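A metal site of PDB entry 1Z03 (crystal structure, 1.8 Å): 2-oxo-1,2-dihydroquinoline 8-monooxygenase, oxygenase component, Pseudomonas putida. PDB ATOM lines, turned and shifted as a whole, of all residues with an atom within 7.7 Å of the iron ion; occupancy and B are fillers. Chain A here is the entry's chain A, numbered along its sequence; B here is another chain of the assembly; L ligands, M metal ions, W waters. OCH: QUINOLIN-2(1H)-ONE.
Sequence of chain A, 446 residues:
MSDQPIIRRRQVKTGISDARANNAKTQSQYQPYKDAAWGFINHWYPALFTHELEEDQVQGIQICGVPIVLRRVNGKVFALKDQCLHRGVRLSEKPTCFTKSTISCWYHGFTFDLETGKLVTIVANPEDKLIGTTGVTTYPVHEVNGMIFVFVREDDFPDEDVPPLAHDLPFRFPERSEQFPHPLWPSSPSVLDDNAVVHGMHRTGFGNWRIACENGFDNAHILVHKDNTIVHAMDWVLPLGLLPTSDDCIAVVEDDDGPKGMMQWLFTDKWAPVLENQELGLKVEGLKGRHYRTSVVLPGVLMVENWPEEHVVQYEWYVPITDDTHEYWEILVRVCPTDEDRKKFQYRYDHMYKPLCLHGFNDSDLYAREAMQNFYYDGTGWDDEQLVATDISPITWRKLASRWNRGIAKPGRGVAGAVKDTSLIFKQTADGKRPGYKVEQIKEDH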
ATOM      1  N   ASN A 215      15.574 -18.049 -13.087  1.00  0.00           N
ATOM      2  CA  ASN A 215      15.566 -16.777 -13.814  1.00  0.00           C
ATOM      3  C   ASN A 215      16.589 -15.744 -13.320  1.00  0.00           C
ATOM      4  O   ASN A 215      17.352 -15.198 -14.109  1.00  0.00           O
ATOM      5  CB  ASN A 215      14.144 -16.195 -13.775  1.00  0.00           C
ATOM      6  CG  ASN A 215      14.066 -14.756 -14.247  1.00  0.00           C
ATOM      7  OD1 ASN A 215      14.421 -13.832 -13.502  1.00  0.00           O
ATOM      8  ND2 ASN A 215      13.613 -14.548 -15.470  1.00  0.00           N
ATOM      9  N   GLY A 216      16.624 -15.530 -12.010  1.00  0.00           N
ATOM     10  CA  GLY A 216      17.490 -14.535 -11.408  1.00  0.00           C
ATOM     11  C   GLY A 216      18.979 -14.505 -11.702  1.00  0.00           C
ATOM     12  O   GLY A 216      19.567 -13.423 -11.784  1.00  0.00           O
ATOM     13  N   PHE A 217      19.611 -15.662 -11.843  1.00  0.00           N
ATOM     14  CA  PHE A 217      21.046 -15.707 -12.098  1.00  0.00           C
ATOM     15  C   PHE A 217      21.394 -16.143 -13.527  1.00  0.00           C
ATOM     16  O   PHE A 217      22.495 -16.619 -13.801  1.00  0.00           O
ATOM     17  CB  PHE A 217      21.748 -16.600 -11.057  1.00  0.00           C
ATOM     18  CG  PHE A 217      21.174 -17.992 -10.957  1.00  0.00           C
ATOM     19  CD1 PHE A 217      21.668 -19.020 -11.763  1.00  0.00           C
ATOM     20  CD2 PHE A 217      20.108 -18.266 -10.095  1.00  0.00           C
ATOM     21  CE1 PHE A 217      21.116 -20.299 -11.704  1.00  0.00           C
ATOM     22  CE2 PHE A 217      19.543 -19.547 -10.030  1.00  0.00           C
ATOM     23  CZ  PHE A 217      20.049 -20.563 -10.839  1.00  0.00           C
ATOM     24  N   ASP A 218      20.438 -15.990 -14.434  1.00  0.00           N
ATOM     25  CA  ASP A 218      20.634 -16.346 -15.834  1.00  0.00           C
ATOM     26  C   ASP A 218      21.094 -15.087 -16.555  1.00  0.00           C
ATOM     27  O   ASP A 218      20.355 -14.105 -16.626  1.00  0.00           O
ATOM     28  CB  ASP A 218      19.328 -16.863 -16.441  1.00  0.00           C
ATOM     29  CG  ASP A 218      19.522 -17.423 -17.847  1.00  0.00           C
ATOM     30  OD1 ASP A 218      19.013 -18.530 -18.114  1.00  0.00           O
ATOM     31  OD2 ASP A 218      20.151 -16.748 -18.688  1.00  0.00           O
ATOM     32  N   HIS A 221      18.976 -13.775 -19.714  1.00  0.00           N
ATOM     33  CA  HIS A 221      17.626 -13.263 -19.490  1.00  0.00           C
ATOM     34  C   HIS A 221      17.523 -11.758 -19.333  1.00  0.00           C
ATOM     35  O   HIS A 221      16.430 -11.197 -19.429  1.00  0.00           O
ATOM     36  CB  HIS A 221      17.000 -13.923 -18.262  1.00  0.00           C
ATOM     37  CG  HIS A 221      17.093 -13.097 -17.014  1.00  0.00           C
ATOM     38  ND1 HIS A 221      18.238 -12.995 -16.260  1.00  0.00           N
ATOM     39  CD2 HIS A 221      16.179 -12.299 -16.408  1.00  0.00           C
ATOM     40  CE1 HIS A 221      18.028 -12.172 -15.256  1.00  0.00           C
ATOM     41  NE2 HIS A 221      16.787 -11.736 -15.317  1.00  0.00           N
ATOM     42  N   ILE A 222      18.652 -11.083 -19.093  1.00  0.00           N
ATOM     43  CA  ILE A 222      18.597  -9.633 -18.887  1.00  0.00           C
ATOM     44  C   ILE A 222      17.997  -8.874 -20.076  1.00  0.00           C
ATOM     45  O   ILE A 222      17.713  -7.682 -19.983  1.00  0.00           O
ATOM     46  CB  ILE A 222      19.981  -9.049 -18.520  1.00  0.00           C
ATOM     47  CG1 ILE A 222      21.044  -9.518 -19.516  1.00  0.00           C
ATOM     48  CG2 ILE A 222      20.341  -9.472 -17.089  1.00  0.00           C
ATOM     49  CD1 ILE A 222      22.439  -8.947 -19.235  1.00  0.00           C
ATOM     50  N   LEU A 223      17.793  -9.576 -21.182  1.00  0.00           N
ATOM     51  CA  LEU A 223      17.178  -8.977 -22.348  1.00  0.00           C
ATOM     52  C   LEU A 223      15.767  -8.505 -21.960  1.00  0.00           C
ATOM     53  O   LEU A 223      15.243  -7.546 -22.516  1.00  0.00           O
ATOM     54  CB  LEU A 223      17.083  -9.998 -23.491  1.00  0.00           C
ATOM     55  CG  LEU A 223      16.419  -9.550 -24.799  1.00  0.00           C
ATOM     56  CD1 LEU A 223      17.229  -8.434 -25.445  1.00  0.00           C
ATOM     57  CD2 LEU A 223      16.330 -10.733 -25.748  1.00  0.00           C
ATOM     58  N   VAL A 224      15.167  -9.211 -20.996  1.00  0.00           N
ATOM     59  CA  VAL A 224      13.819  -8.907 -20.505  1.00  0.00           C
ATOM     60  C   VAL A 224      13.705  -7.483 -19.945  1.00  0.00           C
ATOM     61  O   VAL A 224      12.629  -6.915 -19.913  1.00  0.00           O
ATOM     62  CB  VAL A 224      13.418  -9.884 -19.367  1.00  0.00           C
ATOM     63  CG1 VAL A 224      11.993  -9.659 -18.978  1.00  0.00           C
ATOM     64  CG2 VAL A 224      13.600 -11.301 -19.824  1.00  0.00           C
ATOM     65  N   HIS A 225      14.828  -6.930 -19.506  1.00  0.00           N
ATOM     66  CA  HIS A 225      14.854  -5.590 -18.915  1.00  0.00           C
ATOM     67  C   HIS A 225      15.264  -4.466 -19.861  1.00  0.00           C
ATOM     68  O   HIS A 225      15.360  -3.310 -19.440  1.00  0.00           O
ATOM     69  CB  HIS A 225      15.788  -5.591 -17.706  1.00  0.00           C
ATOM     70  CG  HIS A 225      15.424  -6.622 -16.688  1.00  0.00           C
ATOM     71  ND1 HIS A 225      14.366  -6.475 -15.821  1.00  0.00           N
ATOM     72  CD2 HIS A 225      15.961  -7.837 -16.430  1.00  0.00           C
ATOM     73  CE1 HIS A 225      14.263  -7.559 -15.069  1.00  0.00           C
ATOM     74  NE2 HIS A 225      15.220  -8.394 -15.416  1.00  0.00           N
ATOM     75  N   ASN A 228      13.007  -1.483 -19.351  1.00  0.00           N
ATOM     76  CA  ASN A 228      12.633  -0.997 -18.029  1.00  0.00           C
ATOM     77  C   ASN A 228      12.955   0.480 -17.863  1.00  0.00           C
ATOM     78  O   ASN A 228      14.006   0.944 -18.303  1.00  0.00           O
ATOM     79  CB  ASN A 228      13.321  -1.801 -16.928  1.00  0.00           C
ATOM     80  CG  ASN A 228      12.851  -3.234 -16.876  1.00  0.00           C
ATOM     81  OD1 ASN A 228      11.811  -3.590 -17.433  1.00  0.00           O
ATOM     82  ND2 ASN A 228      13.603  -4.071 -16.196  1.00  0.00           N
ATOM     83  N   GLU A 316      16.724 -12.671  -3.085  1.00  0.00           N
ATOM     84  CA  GLU A 316      15.435 -13.192  -3.511  1.00  0.00           C
ATOM     85  C   GLU A 316      15.314 -14.649  -3.106  1.00  0.00           C
ATOM     86  O   GLU A 316      16.304 -15.384  -3.068  1.00  0.00           O
ATOM     87  CB  GLU A 316      15.264 -13.082  -5.023  1.00  0.00           C
ATOM     88  CG  GLU A 316      15.367 -11.659  -5.575  1.00  0.00           C
ATOM     89  CD  GLU A 316      14.886 -11.536  -7.002  1.00  0.00           C
ATOM     90  OE1 GLU A 316      14.842 -12.568  -7.712  1.00  0.00           O
ATOM     91  OE2 GLU A 316      14.554 -10.420  -7.427  1.00  0.00           O
ATOM     92  N   PHE A 361      11.412  -2.958 -12.655  1.00  0.00           N
ATOM     93  CA  PHE A 361      12.501  -3.832 -13.094  1.00  0.00           C
ATOM     94  C   PHE A 361      12.142  -5.307 -12.880  1.00  0.00           C
ATOM     95  O   PHE A 361      12.076  -6.087 -13.833  1.00  0.00           O
ATOM     96  CB  PHE A 361      13.804  -3.517 -12.351  1.00  0.00           C
ATOM     97  CG  PHE A 361      15.010  -4.221 -12.914  1.00  0.00           C
ATOM     98  CD1 PHE A 361      15.688  -3.705 -14.015  1.00  0.00           C
ATOM     99  CD2 PHE A 361      15.459  -5.421 -12.367  1.00  0.00           C
ATOM    100  CE1 PHE A 361      16.791  -4.372 -14.563  1.00  0.00           C
ATOM    101  CE2 PHE A 361      16.559  -6.091 -12.907  1.00  0.00           C
ATOM    102  CZ  PHE A 361      17.214  -5.567 -14.003  1.00  0.00           C
ATOM    103  N   ASN A 362      11.886  -5.685 -11.633  1.00  0.00           N
ATOM    104  CA  ASN A 362      11.571  -7.089 -11.342  1.00  0.00           C
ATOM    105  C   ASN A 362      10.186  -7.574 -11.741  1.00  0.00           C
ATOM    106  O   ASN A 362       9.961  -8.782 -11.817  1.00  0.00           O
ATOM    107  CB  ASN A 362      11.828  -7.376  -9.873  1.00  0.00           C
ATOM    108  CG  ASN A 362      13.318  -7.420  -9.540  1.00  0.00           C
ATOM    109  OD1 ASN A 362      13.820  -6.586  -8.783  1.00  0.00           O
ATOM    110  ND2 ASN A 362      14.025  -8.389 -10.121  1.00  0.00           N
ATOM    111  N   ASP A 363       9.249  -6.668 -11.992  1.00  0.00           N
ATOM    112  CA  ASP A 363       7.922  -7.093 -12.410  1.00  0.00           C
ATOM    113  C   ASP A 363       8.038  -7.840 -13.736  1.00  0.00           C
ATOM    114  O   ASP A 363       7.269  -8.748 -14.008  1.00  0.00           O
ATOM    115  CB  ASP A 363       6.979  -5.902 -12.551  1.00  0.00           C
ATOM    116  CG  ASP A 363       6.405  -5.431 -11.209  1.00  0.00           C
ATOM    117  OD1 ASP A 363       5.825  -4.330 -11.172  1.00  0.00           O
ATOM    118  OD2 ASP A 363       6.537  -6.162 -10.198  1.00  0.00           O
ATOM    119  N   SER A 364       9.011  -7.451 -14.561  1.00  0.00           N
ATOM    120  CA  SER A 364       9.228  -8.103 -15.850  1.00  0.00           C
ATOM    121  C   SER A 364       9.569  -9.574 -15.648  1.00  0.00           C
ATOM    122  O   SER A 364       9.194 -10.425 -16.460  1.00  0.00           O
ATOM    123  CB  SER A 364      10.373  -7.442 -16.612  1.00  0.00           C
ATOM    124  OG  SER A 364      10.074  -6.109 -16.973  1.00  0.00           O
ATOM    125  N   ASP A 365      10.296  -9.876 -14.577  1.00  0.00           N
ATOM    126  CA  ASP A 365      10.683 -11.254 -14.249  1.00  0.00           C
ATOM    127  C   ASP A 365       9.472 -12.073 -13.811  1.00  0.00           C
ATOM    128  O   ASP A 365       9.414 -13.283 -14.045  1.00  0.00           O
ATOM    129  CB  ASP A 365      11.724 -11.268 -13.124  1.00  0.00           C
ATOM    130  CG  ASP A 365      13.024 -10.600 -13.532  1.00  0.00           C
ATOM    131  OD1 ASP A 365      13.462  -9.641 -12.868  1.00  0.00           O
ATOM    132  OD2 ASP A 365      13.590 -11.055 -14.546  1.00  0.00           O
ATOM    133  N   LEU A 366       8.532 -11.400 -13.157  1.00  0.00           N
ATOM    134  CA  LEU A 366       7.312 -12.034 -12.678  1.00  0.00           C
ATOM    135  C   LEU A 366       6.620 -12.769 -13.820  1.00  0.00           C
ATOM    136  O   LEU A 366       6.332 -13.956 -13.729  1.00  0.00           O
ATOM    137  CB  LEU A 366       6.365 -10.973 -12.120  1.00  0.00           C
ATOM    138  CG  LEU A 366       5.644 -11.238 -10.811  1.00  0.00           C
ATOM    139  CD1 LEU A 366       4.590 -10.162 -10.595  1.00  0.00           C
ATOM    140  CD2 LEU A 366       4.997 -12.598 -10.862  1.00  0.00           C
ATOM    141  N   ALA A 368       7.851 -13.258 -16.934  1.00  0.00           N
ATOM    142  CA  ALA A 368       8.769 -14.120 -17.685  1.00  0.00           C
ATOM    143  C   ALA A 368       8.745 -15.523 -17.089  1.00  0.00           C
ATOM    144  O   ALA A 368       8.648 -16.512 -17.831  1.00  0.00           O
ATOM    145  CB  ALA A 368      10.188 -13.551 -17.636  1.00  0.00           C
ATOM    146  N   ARG A 369       8.823 -15.606 -15.758  1.00  0.00           N
ATOM    147  CA  ARG A 369       8.818 -16.887 -15.049  1.00  0.00           C
ATOM    148  C   ARG A 369       7.502 -17.625 -15.275  1.00  0.00           C
ATOM    149  O   ARG A 369       7.491 -18.833 -15.491  1.00  0.00           O
ATOM    150  CB  ARG A 369       8.985 -16.687 -13.552  1.00  0.00           C
ATOM    151  CG  ARG A 369      10.236 -15.975 -13.126  1.00  0.00           C
ATOM    152  CD  ARG A 369      10.106 -15.570 -11.679  1.00  0.00           C
ATOM    153  NE  ARG A 369      11.226 -14.739 -11.252  1.00  0.00           N
ATOM    154  CZ  ARG A 369      11.115 -13.772 -10.352  1.00  0.00           C
ATOM    155  NH1 ARG A 369      12.186 -13.061 -10.015  1.00  0.00           N
ATOM    156  NH2 ARG A 369       9.935 -13.504  -9.796  1.00  0.00           N
ATOM    157  N   TYR B 107      12.377 -13.516 -24.149  1.00  0.00           N
ATOM    158  CA  TYR B 107      13.057 -13.963 -22.944  1.00  0.00           C
ATOM    159  C   TYR B 107      14.573 -14.030 -23.044  1.00  0.00           C
ATOM    160  O   TYR B 107      15.264 -13.276 -22.356  1.00  0.00           O
ATOM    161  CB  TYR B 107      12.482 -15.310 -22.506  1.00  0.00           C
ATOM    162  CG  TYR B 107      12.618 -15.601 -21.028  1.00  0.00           C
ATOM    163  CD1 TYR B 107      11.944 -16.677 -20.463  1.00  0.00           C
ATOM    164  CD2 TYR B 107      13.390 -14.797 -20.190  1.00  0.00           C
ATOM    165  CE1 TYR B 107      12.040 -16.958 -19.107  1.00  0.00           C
ATOM    166  CE2 TYR B 107      13.493 -15.058 -18.826  1.00  0.00           C
ATOM    167  CZ  TYR B 107      12.813 -16.147 -18.300  1.00  0.00           C
ATOM    168  OH  TYR B 107      12.899 -16.429 -16.948  1.00  0.00           O
HETATM  169  O1  OCH L   1      21.370 -11.305 -13.638  1.00  0.00           O
HETATM  170  N2  OCH L   1      19.926 -10.801 -11.888  1.00  0.00           N
HETATM  171  C3  OCH L   1      19.243  -9.880 -11.058  1.00  0.00           C
HETATM  172  C4  OCH L   1      18.367 -10.327 -10.003  1.00  0.00           C
HETATM  173  C5  OCH L   1      17.716  -9.370  -9.229  1.00  0.00           C
HETATM  174  C6  OCH L   1      17.899  -7.968  -9.482  1.00  0.00           C
HETATM  175  C7  OCH L   1      18.740  -7.533 -10.499  1.00  0.00           C
HETATM  176  C8  OCH L   1      19.427  -8.447 -11.314  1.00  0.00           C
HETATM  177  C9  OCH L   1      20.323  -8.009 -12.419  1.00  0.00           C
HETATM  178  C10 OCH L   1      20.970  -8.895 -13.188  1.00  0.00           C
HETATM  179  C1  OCH L   1      20.817 -10.429 -12.977  1.00  0.00           C
HETATM  180 FE    FE M   1      15.524 -10.177 -14.440  1.00  0.00          FE
HETATM  181  O   HOH W   1      15.971 -10.206 -11.910  1.00  0.00           O
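The backbone carbonyl oxygen (O) of Gly 216 sits at hydrogen-bond distance from a nitrogen (N2) of the ligand, 2.6 Å away.
ND1 of His 225 is in hydrogen-bond range of ND2 of Asn 228 (2.5 Å). A ring nitrogen (ND1) of His 221 lies within hydrogen-bond range of the backbone carbonyl oxygen (O) of Asp 218 (2.4 Å). ND1 of His 225 sits close to O of Phe 361. ND1 of His 221 sits at hydrogen-bond distance from O of Asn 215, at 3.2 Å. OD1 of Asp 365 is in hydrogen-bond range of ND2 of Asn 362 (3.1 Å). OD1 of Asn 215 sits close to OD2 of Asp 365 (3.1 Å). The side-chain amide nitrogen of Asn 215 is in hydrogen-bond range of the side-chain hydroxyl of Tyr 107 of chain B.
Residues that only touch the iron ion: Asn 215 (3.9 Å). Four residues have an atom within 4 Å of the iron ion: Asn 215, His 221, His 225 and Asp 365.
A ring nitrogen (NE2) of His 225 is bound to the iron ion (2.1 Å). OD2 of Asp 365 is bound to the iron ion (2.1 Å). NE2 of His 221 is bound to the iron ion (2.2 Å). The iron ion is bound by water W1, 2.6 Å away. Slightly farther from the iron ion lies the side-chain carboxylate (OD1) of Asp 365 (2.6 Å).
Water W1 bridges the side-chain carboxylate of Asp 365 (2.7 Å) and the side-chain amide nitrogen of Asn 362 (3.2 Å).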
